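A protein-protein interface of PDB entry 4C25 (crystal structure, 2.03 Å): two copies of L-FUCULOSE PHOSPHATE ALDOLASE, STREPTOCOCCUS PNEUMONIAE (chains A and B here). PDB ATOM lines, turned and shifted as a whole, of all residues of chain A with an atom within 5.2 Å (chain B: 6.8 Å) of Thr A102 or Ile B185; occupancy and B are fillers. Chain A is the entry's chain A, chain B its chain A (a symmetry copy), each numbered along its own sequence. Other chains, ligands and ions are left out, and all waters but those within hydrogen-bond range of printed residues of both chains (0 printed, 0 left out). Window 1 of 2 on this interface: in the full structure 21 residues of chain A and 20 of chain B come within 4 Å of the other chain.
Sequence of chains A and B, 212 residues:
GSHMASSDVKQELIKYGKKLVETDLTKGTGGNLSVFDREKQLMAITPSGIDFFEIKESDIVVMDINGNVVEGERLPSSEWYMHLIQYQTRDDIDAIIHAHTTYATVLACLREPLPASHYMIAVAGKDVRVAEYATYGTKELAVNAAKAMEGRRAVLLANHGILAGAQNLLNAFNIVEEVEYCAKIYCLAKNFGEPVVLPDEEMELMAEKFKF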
ATOM      1  N   LEU A  25     -21.424  -3.755  -5.020  1.00  0.00           N
ATOM      2  CA  LEU A  25     -22.189  -4.894  -4.512  1.00  0.00           C
ATOM      3  C   LEU A  25     -21.300  -5.626  -3.547  1.00  0.00           C
ATOM      4  O   LEU A  25     -21.718  -6.002  -2.449  1.00  0.00           O
ATOM      5  CB  LEU A  25     -22.642  -5.832  -5.627  1.00  0.00           C
ATOM      6  CG  LEU A  25     -24.072  -5.652  -6.126  1.00  0.00           C
ATOM      7  CD1 LEU A  25     -24.287  -6.536  -7.347  1.00  0.00           C
ATOM      8  CD2 LEU A  25     -25.083  -5.962  -5.018  1.00  0.00           C
ATOM      9  N   HIS A 100     -20.123 -11.758  -1.329  1.00  0.00           N
ATOM     10  CA  HIS A 100     -20.381 -11.337   0.056  1.00  0.00           C
ATOM     11  C   HIS A 100     -20.910  -9.897   0.019  1.00  0.00           C
ATOM     12  O   HIS A 100     -20.124  -8.932   0.005  1.00  0.00           O
ATOM     13  CB  HIS A 100     -19.111 -11.400   0.915  1.00  0.00           C
ATOM     14  CG  HIS A 100     -18.384 -12.710   0.842  1.00  0.00           C
ATOM     15  ND1 HIS A 100     -17.167 -12.914   1.453  1.00  0.00           N
ATOM     16  CD2 HIS A 100     -18.683 -13.869   0.206  1.00  0.00           C
ATOM     17  CE1 HIS A 100     -16.748 -14.138   1.199  1.00  0.00           C
ATOM     18  NE2 HIS A 100     -17.645 -14.736   0.436  1.00  0.00           N
ATOM     19  N   THR A 101     -22.233  -9.763  -0.049  1.00  0.00           N
ATOM     20  CA  THR A 101     -22.866  -8.449  -0.183  1.00  0.00           C
ATOM     21  C   THR A 101     -23.186  -7.996   1.249  1.00  0.00           C
ATOM     22  O   THR A 101     -22.702  -8.612   2.199  1.00  0.00           O
ATOM     23  CB  THR A 101     -24.121  -8.501  -1.086  1.00  0.00           C
ATOM     24  OG1 THR A 101     -25.084  -9.399  -0.514  1.00  0.00           O
ATOM     25  CG2 THR A 101     -23.769  -8.966  -2.514  1.00  0.00           C
ATOM     26  N   THR A 102     -24.002  -6.966   1.434  1.00  0.00           N
ATOM     27  CA  THR A 102     -24.230  -6.497   2.788  1.00  0.00           C
ATOM     28  C   THR A 102     -25.437  -7.146   3.516  1.00  0.00           C
ATOM     29  O   THR A 102     -25.274  -7.980   4.423  1.00  0.00           O
ATOM     30  CB  THR A 102     -24.280  -4.948   2.787  1.00  0.00           C
ATOM     31  OG1 THR A 102     -23.140  -4.470   2.065  1.00  0.00           O
ATOM     32  CG2 THR A 102     -24.220  -4.399   4.173  1.00  0.00           C
ATOM     33  N   TYR A 103     -26.642  -6.775   3.110  1.00  0.00           N
ATOM     34  CA  TYR A 103     -27.852  -7.165   3.862  1.00  0.00           C
ATOM     35  C   TYR A 103     -28.244  -8.648   3.631  1.00  0.00           C
ATOM     36  O   TYR A 103     -28.813  -9.288   4.514  1.00  0.00           O
ATOM     37  CB  TYR A 103     -29.008  -6.152   3.579  1.00  0.00           C
ATOM     38  CG  TYR A 103     -28.782  -4.774   4.264  1.00  0.00           C
ATOM     39  CD1 TYR A 103     -28.034  -3.745   3.631  1.00  0.00           C
ATOM     40  CD2 TYR A 103     -29.286  -4.530   5.542  1.00  0.00           C
ATOM     41  CE1 TYR A 103     -27.816  -2.514   4.275  1.00  0.00           C
ATOM     42  CE2 TYR A 103     -29.081  -3.316   6.172  1.00  0.00           C
ATOM     43  CZ  TYR A 103     -28.350  -2.295   5.541  1.00  0.00           C
ATOM     44  OH  TYR A 103     -28.140  -1.064   6.203  1.00  0.00           O
ATOM     45  N   ALA A 104     -27.936  -9.195   2.464  1.00  0.00           N
ATOM     46  CA  ALA A 104     -28.145 -10.646   2.219  1.00  0.00           C
ATOM     47  C   ALA A 104     -27.280 -11.465   3.186  1.00  0.00           C
ATOM     48  O   ALA A 104     -27.732 -12.386   3.890  1.00  0.00           O
ATOM     49  CB  ALA A 104     -27.793 -11.004   0.779  1.00  0.00           C
ATOM     50  N   THR A 105     -26.034 -11.063   3.267  1.00  0.00           N
ATOM     51  CA  THR A 105     -25.105 -11.638   4.218  1.00  0.00           C
ATOM     52  C   THR A 105     -25.510 -11.461   5.666  1.00  0.00           C
ATOM     53  O   THR A 105     -25.217 -12.317   6.489  1.00  0.00           O
ATOM     54  CB  THR A 105     -23.756 -11.014   3.973  1.00  0.00           C
ATOM     55  OG1 THR A 105     -23.406 -11.321   2.625  1.00  0.00           O
ATOM     56  CG2 THR A 105     -22.747 -11.602   4.883  1.00  0.00           C
ATOM     57  N   VAL A 106     -26.132 -10.329   5.981  1.00  0.00           N
ATOM     58  CA  VAL A 106     -26.709 -10.094   7.291  1.00  0.00           C
ATOM     59  C   VAL A 106     -27.784 -11.120   7.595  1.00  0.00           C
ATOM     60  O   VAL A 106     -27.836 -11.686   8.689  1.00  0.00           O
ATOM     61  CB  VAL A 106     -27.313  -8.684   7.365  1.00  0.00           C
ATOM     62  CG1 VAL A 106     -28.075  -8.496   8.686  1.00  0.00           C
ATOM     63  CG2 VAL A 106     -26.215  -7.658   7.282  1.00  0.00           C
ATOM     64  N   CYS A 109     -26.104 -14.437   8.209  1.00  0.00           N
ATOM     65  CA  CYS A 109     -25.463 -14.662   9.519  1.00  0.00           C
ATOM     66  C   CYS A 109     -26.478 -14.833  10.657  1.00  0.00           C
ATOM     67  O   CYS A 109     -26.127 -15.239  11.763  1.00  0.00           O
ATOM     68  CB  CYS A 109     -24.461 -13.562   9.851  1.00  0.00           C
ATOM     69  SG  CYS A 109     -23.162 -13.370   8.599  1.00  0.00           S
ATOM     70  N   GLU A 180     -29.996  -8.560  -3.153  1.00  0.00           N
ATOM     71  CA  GLU A 180     -29.381  -7.676  -2.143  1.00  0.00           C
ATOM     72  C   GLU A 180     -30.301  -6.479  -1.806  1.00  0.00           C
ATOM     73  O   GLU A 180     -30.384  -6.015  -0.669  1.00  0.00           O
ATOM     74  CB  GLU A 180     -27.963  -7.204  -2.579  1.00  0.00           C
ATOM     75  CG  GLU A 180     -27.315  -6.133  -1.675  1.00  0.00           C
ATOM     76  CD  GLU A 180     -27.224  -6.543  -0.198  1.00  0.00           C
ATOM     77  OE1 GLU A 180     -27.267  -7.775   0.137  1.00  0.00           O
ATOM     78  OE2 GLU A 180     -27.110  -5.620   0.648  1.00  0.00           O
ATOM     79  N   TYR B 103     -18.644   1.134  11.438  1.00  0.00           N
ATOM     80  CA  TYR B 103     -19.273   0.150  12.344  1.00  0.00           C
ATOM     81  C   TYR B 103     -18.274  -0.428  13.380  1.00  0.00           C
ATOM     82  O   TYR B 103     -18.664  -0.786  14.490  1.00  0.00           O
ATOM     83  CB  TYR B 103     -20.027  -0.937  11.513  1.00  0.00           C
ATOM     84  CG  TYR B 103     -21.334  -0.400  10.864  1.00  0.00           C
ATOM     85  CD1 TYR B 103     -21.324   0.235   9.592  1.00  0.00           C
ATOM     86  CD2 TYR B 103     -22.551  -0.501  11.538  1.00  0.00           C
ATOM     87  CE1 TYR B 103     -22.509   0.740   9.030  1.00  0.00           C
ATOM     88  CE2 TYR B 103     -23.720  -0.014  10.981  1.00  0.00           C
ATOM     89  CZ  TYR B 103     -23.710   0.604   9.719  1.00  0.00           C
ATOM     90  OH  TYR B 103     -24.912   1.106   9.169  1.00  0.00           O
ATOM     91  N   LEU B 114     -15.952  -7.709  18.611  1.00  0.00           N
ATOM     92  CA  LEU B 114     -16.507  -8.288  17.393  1.00  0.00           C
ATOM     93  C   LEU B 114     -16.306  -9.816  17.432  1.00  0.00           C
ATOM     94  O   LEU B 114     -15.155 -10.271  17.346  1.00  0.00           O
ATOM     95  CB  LEU B 114     -15.809  -7.659  16.168  1.00  0.00           C
ATOM     96  CG  LEU B 114     -16.191  -8.045  14.738  1.00  0.00           C
ATOM     97  CD1 LEU B 114     -17.681  -7.985  14.562  1.00  0.00           C
ATOM     98  CD2 LEU B 114     -15.470  -7.239  13.660  1.00  0.00           C
ATOM     99  N   SER B 117     -19.598 -13.978  13.896  1.00  0.00           N
ATOM    100  CA  SER B 117     -20.829 -14.075  13.134  1.00  0.00           C
ATOM    101  C   SER B 117     -20.509 -14.181  11.643  1.00  0.00           C
ATOM    102  O   SER B 117     -21.268 -14.795  10.911  1.00  0.00           O
ATOM    103  CB  SER B 117     -21.739 -12.871  13.417  1.00  0.00           C
ATOM    104  OG  SER B 117     -20.984 -11.649  13.401  1.00  0.00           O
ATOM    105  N   HIS B 118     -19.397 -13.602  11.191  1.00  0.00           N
ATOM    106  CA  HIS B 118     -18.908 -13.860   9.819  1.00  0.00           C
ATOM    107  C   HIS B 118     -17.498 -14.441   9.844  1.00  0.00           C
ATOM    108  O   HIS B 118     -16.626 -13.974  10.577  1.00  0.00           O
ATOM    109  CB  HIS B 118     -18.913 -12.592   8.962  1.00  0.00           C
ATOM    110  CG  HIS B 118     -18.860 -12.868   7.488  1.00  0.00           C
ATOM    111  ND1 HIS B 118     -17.702 -13.231   6.844  1.00  0.00           N
ATOM    112  CD2 HIS B 118     -19.833 -12.865   6.542  1.00  0.00           C
ATOM    113  CE1 HIS B 118     -17.951 -13.422   5.558  1.00  0.00           C
ATOM    114  NE2 HIS B 118     -19.238 -13.203   5.345  1.00  0.00           N
ATOM    115  N   GLU B 180     -13.903  -3.990   9.219  1.00  0.00           N
ATOM    116  CA  GLU B 180     -15.025  -3.037   9.111  1.00  0.00           C
ATOM    117  C   GLU B 180     -16.280  -3.708   8.505  1.00  0.00           C
ATOM    118  O   GLU B 180     -17.419  -3.426   8.876  1.00  0.00           O
ATOM    119  CB  GLU B 180     -14.619  -1.759   8.319  1.00  0.00           C
ATOM    120  CG  GLU B 180     -15.775  -0.786   7.997  1.00  0.00           C
ATOM    121  CD  GLU B 180     -16.559  -0.325   9.234  1.00  0.00           C
ATOM    122  OE1 GLU B 180     -16.032  -0.389  10.397  1.00  0.00           O
ATOM    123  OE2 GLU B 180     -17.724   0.107   9.048  1.00  0.00           O
ATOM    124  N   TYR B 181     -16.057  -4.615   7.583  1.00  0.00           N
ATOM    125  CA  TYR B 181     -17.160  -5.261   6.929  1.00  0.00           C
ATOM    126  C   TYR B 181     -17.844  -6.204   7.908  1.00  0.00           C
ATOM    127  O   TYR B 181     -19.068  -6.243   7.979  1.00  0.00           O
ATOM    128  CB  TYR B 181     -16.662  -5.965   5.688  1.00  0.00           C
ATOM    129  CG  TYR B 181     -17.653  -6.919   5.074  1.00  0.00           C
ATOM    130  CD1 TYR B 181     -18.694  -6.449   4.241  1.00  0.00           C
ATOM    131  CD2 TYR B 181     -17.551  -8.300   5.302  1.00  0.00           C
ATOM    132  CE1 TYR B 181     -19.603  -7.339   3.659  1.00  0.00           C
ATOM    133  CE2 TYR B 181     -18.429  -9.184   4.717  1.00  0.00           C
ATOM    134  CZ  TYR B 181     -19.457  -8.701   3.903  1.00  0.00           C
ATOM    135  OH  TYR B 181     -20.356  -9.596   3.366  1.00  0.00           O
ATOM    136  N   CYS B 182     -17.059  -6.941   8.673  1.00  0.00           N
ATOM    137  CA  CYS B 182     -17.588  -7.875   9.663  1.00  0.00           C
ATOM    138  C   CYS B 182     -18.322  -7.191  10.801  1.00  0.00           C
ATOM    139  O   CYS B 182     -19.348  -7.666  11.282  1.00  0.00           O
ATOM    140  CB  CYS B 182     -16.437  -8.692  10.241  1.00  0.00           C
ATOM    141  SG  CYS B 182     -15.856 -10.011   9.162  1.00  0.00           S
ATOM    142  N   ALA B 183     -17.772  -6.066  11.260  1.00  0.00           N
ATOM    143  CA  ALA B 183     -18.425  -5.240  12.286  1.00  0.00           C
ATOM    144  C   ALA B 183     -19.755  -4.734  11.708  1.00  0.00           C
ATOM    145  O   ALA B 183     -20.811  -4.767  12.389  1.00  0.00           O
ATOM    146  CB  ALA B 183     -17.532  -4.057  12.657  1.00  0.00           C
ATOM    147  N   LYS B 184     -19.701  -4.263  10.464  1.00  0.00           N
ATOM    148  CA  LYS B 184     -20.963  -3.824   9.824  1.00  0.00           C
ATOM    149  C   LYS B 184     -21.980  -4.939   9.833  1.00  0.00           C
ATOM    150  O   LYS B 184     -23.070  -4.765  10.405  1.00  0.00           O
ATOM    151  CB  LYS B 184     -20.776  -3.311   8.410  1.00  0.00           C
ATOM    152  CG  LYS B 184     -22.044  -2.687   7.868  1.00  0.00           C
ATOM    153  CD  LYS B 184     -21.798  -1.998   6.541  1.00  0.00           C
ATOM    154  CE  LYS B 184     -23.119  -1.489   5.998  1.00  0.00           C
ATOM    155  NZ  LYS B 184     -22.833  -0.411   5.009  1.00  0.00           N
ATOM    156  N   ILE B 185     -21.620  -6.091   9.227  1.00  0.00           N
ATOM    157  CA  ILE B 185     -22.474  -7.260   9.293  1.00  0.00           C
ATOM    158  C   ILE B 185     -23.030  -7.499  10.728  1.00  0.00           C
ATOM    159  O   ILE B 185     -24.207  -7.734  10.925  1.00  0.00           O
ATOM    160  CB  ILE B 185     -21.741  -8.525   8.806  1.00  0.00           C
ATOM    161  CG1 ILE B 185     -21.181  -8.370   7.367  1.00  0.00           C
ATOM    162  CG2 ILE B 185     -22.633  -9.751   8.937  1.00  0.00           C
ATOM    163  CD1 ILE B 185     -22.189  -7.900   6.330  1.00  0.00           C
ATOM    164  N   TYR B 186     -22.158  -7.471  11.720  1.00  0.00           N
ATOM    165  CA  TYR B 186     -22.539  -7.900  13.065  1.00  0.00           C
ATOM    166  C   TYR B 186     -23.541  -6.932  13.700  1.00  0.00           C
ATOM    167  O   TYR B 186     -24.519  -7.338  14.306  1.00  0.00           O
ATOM    168  CB  TYR B 186     -21.277  -8.109  13.916  1.00  0.00           C
ATOM    169  CG  TYR B 186     -21.526  -8.356  15.425  1.00  0.00           C
ATOM    170  CD1 TYR B 186     -22.273  -9.453  15.863  1.00  0.00           C
ATOM    171  CD2 TYR B 186     -21.003  -7.502  16.391  1.00  0.00           C
ATOM    172  CE1 TYR B 186     -22.495  -9.691  17.222  1.00  0.00           C
ATOM    173  CE2 TYR B 186     -21.217  -7.717  17.759  1.00  0.00           C
ATOM    174  CZ  TYR B 186     -21.967  -8.806  18.165  1.00  0.00           C
ATOM    175  OH  TYR B 186     -22.162  -9.048  19.490  1.00  0.00           O
ATOM    176  N   CYS B 187     -23.302  -5.641  13.563  1.00  0.00           N
ATOM    177  CA  CYS B 187     -24.242  -4.623  14.054  1.00  0.00           C
ATOM    178  C   CYS B 187     -25.611  -4.752  13.393  1.00  0.00           C
ATOM    179  O   CYS B 187     -26.660  -4.824  14.093  1.00  0.00           O
ATOM    180  CB  CYS B 187     -23.672  -3.224  13.820  1.00  0.00           C
ATOM    181  SG  CYS B 187     -22.135  -2.924  14.725  1.00  0.00           S
ATOM    182  N   LEU B 188     -25.611  -4.832  12.058  1.00  0.00           N
ATOM    183  CA  LEU B 188     -26.886  -4.922  11.334  1.00  0.00           C
ATOM    184  C   LEU B 188     -27.659  -6.161  11.751  1.00  0.00           C
ATOM    185  O   LEU B 188     -28.877  -6.077  11.980  1.00  0.00           O
ATOM    186  CB  LEU B 188     -26.703  -4.893   9.826  1.00  0.00           C
ATOM    187  CG  LEU B 188     -25.860  -3.755   9.192  1.00  0.00           C
ATOM    188  CD1 LEU B 188     -25.623  -3.904   7.671  1.00  0.00           C
ATOM    189  CD2 LEU B 188     -26.356  -2.334   9.522  1.00  0.00           C
ATOM    190  N   ALA B 189     -26.961  -7.304  11.872  1.00  0.00           N
ATOM    191  CA  ALA B 189     -27.615  -8.545  12.272  1.00  0.00           C
ATOM    192  C   ALA B 189     -28.276  -8.341  13.607  1.00  0.00           C
ATOM    193  O   ALA B 189     -29.357  -8.853  13.852  1.00  0.00           O
ATOM    194  CB  ALA B 189     -26.598  -9.689  12.373  1.00  0.00           C
ATOM    195  N   LYS B 190     -27.587  -7.615  14.486  1.00  0.00           N
ATOM    196  CA  LYS B 190     -28.026  -7.486  15.877  1.00  0.00           C
ATOM    197  C   LYS B 190     -29.252  -6.568  15.951  1.00  0.00           C
ATOM    198  O   LYS B 190     -30.033  -6.642  16.901  1.00  0.00           O
ATOM    199  CB  LYS B 190     -26.856  -7.000  16.745  1.00  0.00           C
ATOM    200  CG  LYS B 190     -27.181  -6.806  18.213  1.00  0.00           C
ATOM    201  CD  LYS B 190     -26.644  -7.935  19.084  1.00  0.00           C
ATOM    202  CE  LYS B 190     -27.234  -7.815  20.489  1.00  0.00           C
ATOM    203  NZ  LYS B 190     -26.445  -8.573  21.504  1.00  0.00           N
ATOM    204  N   PRO B 195     -27.410 -12.585  16.040  1.00  0.00           N
ATOM    205  CA  PRO B 195     -26.418 -13.116  15.089  1.00  0.00           C
ATOM    206  C   PRO B 195     -25.849 -14.473  15.572  1.00  0.00           C
ATOM    207  O   PRO B 195     -25.589 -14.639  16.760  1.00  0.00           O
ATOM    208  CB  PRO B 195     -25.319 -12.039  15.078  1.00  0.00           C
ATOM    209  CG  PRO B 195     -25.932 -10.821  15.656  1.00  0.00           C
ATOM    210  CD  PRO B 195     -27.007 -11.281  16.601  1.00  0.00           C
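Thr A102 touches just these residues of chain B: Lys B184 (3.6 Å), Ile B185 (3.6 Å) and Leu B188 (3.8 Å).
Printed residues of chain A within 4 Å of Ile B185: Thr A102 and Cys A109.
Of the printed residues of chain B, Val A106 touches Leu B188 (3.8 Å) and Ala B189 (3.6 Å).
Of the printed residues of chain B, His A100 touches Tyr B181.
Leu A25 touches none of the printed residues of chain B.
The nearest printed residue of chain A that does not touch Ile B185 is Thr A105 (4.01 Å).
The nearest printed residue of chain A that does not touch Tyr B181 is Thr A102 (4.8 Å).
Among the printed residues, pairs that only touch across the chains: Thr A102 with Lys B184 (3.6 Å), Thr A102 with Ile B185 (3.6 Å), Thr A102 with Leu B188 (3.8 Å), Tyr A103 with Leu B188 (3.8 Å), Thr A105 with His B118 (3.6 Å), Thr A105 with Tyr B181 (3.5 Å), Val A106 with Leu B188 (3.8 Å), Val A106 with Ala B189 (3.6 Å), Cys A109 with His B118 (3.9 Å), Cys A109 with Ile B185 (3.7 Å) and Cys A109 with Pro B195 (3.9 Å).
The backbone carbonyl oxygen (O) of Thr A101 sits at hydrogen-bond distance from the side-chain hydroxyl (OG1) of Thr A105.
The side-chain carboxylate (OE1) of Glu A180 sits at hydrogen-bond distance from the side-chain hydroxyl (OG1) of Thr A101.
The backbone NH (N) of Thr A102 is in hydrogen-bond range of the side-chain carboxylate (OE2) of Glu A180.
The side-chain carboxylate (OE2) of Glu A180 lies within hydrogen-bond range of the backbone NH (N) of Tyr A103 (2.8 Å).
The backbone carbonyl oxygen (O) of Thr A105 is in hydrogen-bond range of the side-chain sulfur (SG) of Cys A109 (3.1 Å).
Of the 16 printed residues of chain B, 8 touch a printed residue of chain A.
Hydrophobic or aromatic side chains of chain B that line the printed part of chain A: His B118, Tyr B181, Ile B185 and Leu B188.
Of the 10 printed residues of chain A, 7 touch a printed residue of chain B.
Among the printed residues, no Asp or Glu carboxylate lies within 4 Å of a Lys or Arg side-chain nitrogen of the other chain.
O of His A100 sits close to OH of Tyr B181.
The backbone carbonyl oxygen (O) of Thr A101 lies within hydrogen-bond range of the side-chain hydroxyl (OH) of Tyr B181, at 2.8 Å.
The side-chain sulfur (SG) of Cys A109 is in hydrogen-bond range of the backbone carbonyl oxygen (O) of Ser B117 (3.3 Å).
2 positions are printed for both chains.
Of the 14 pairs that touch across the chains among the printed residues, none has its exchanged pair printed and touching as well.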
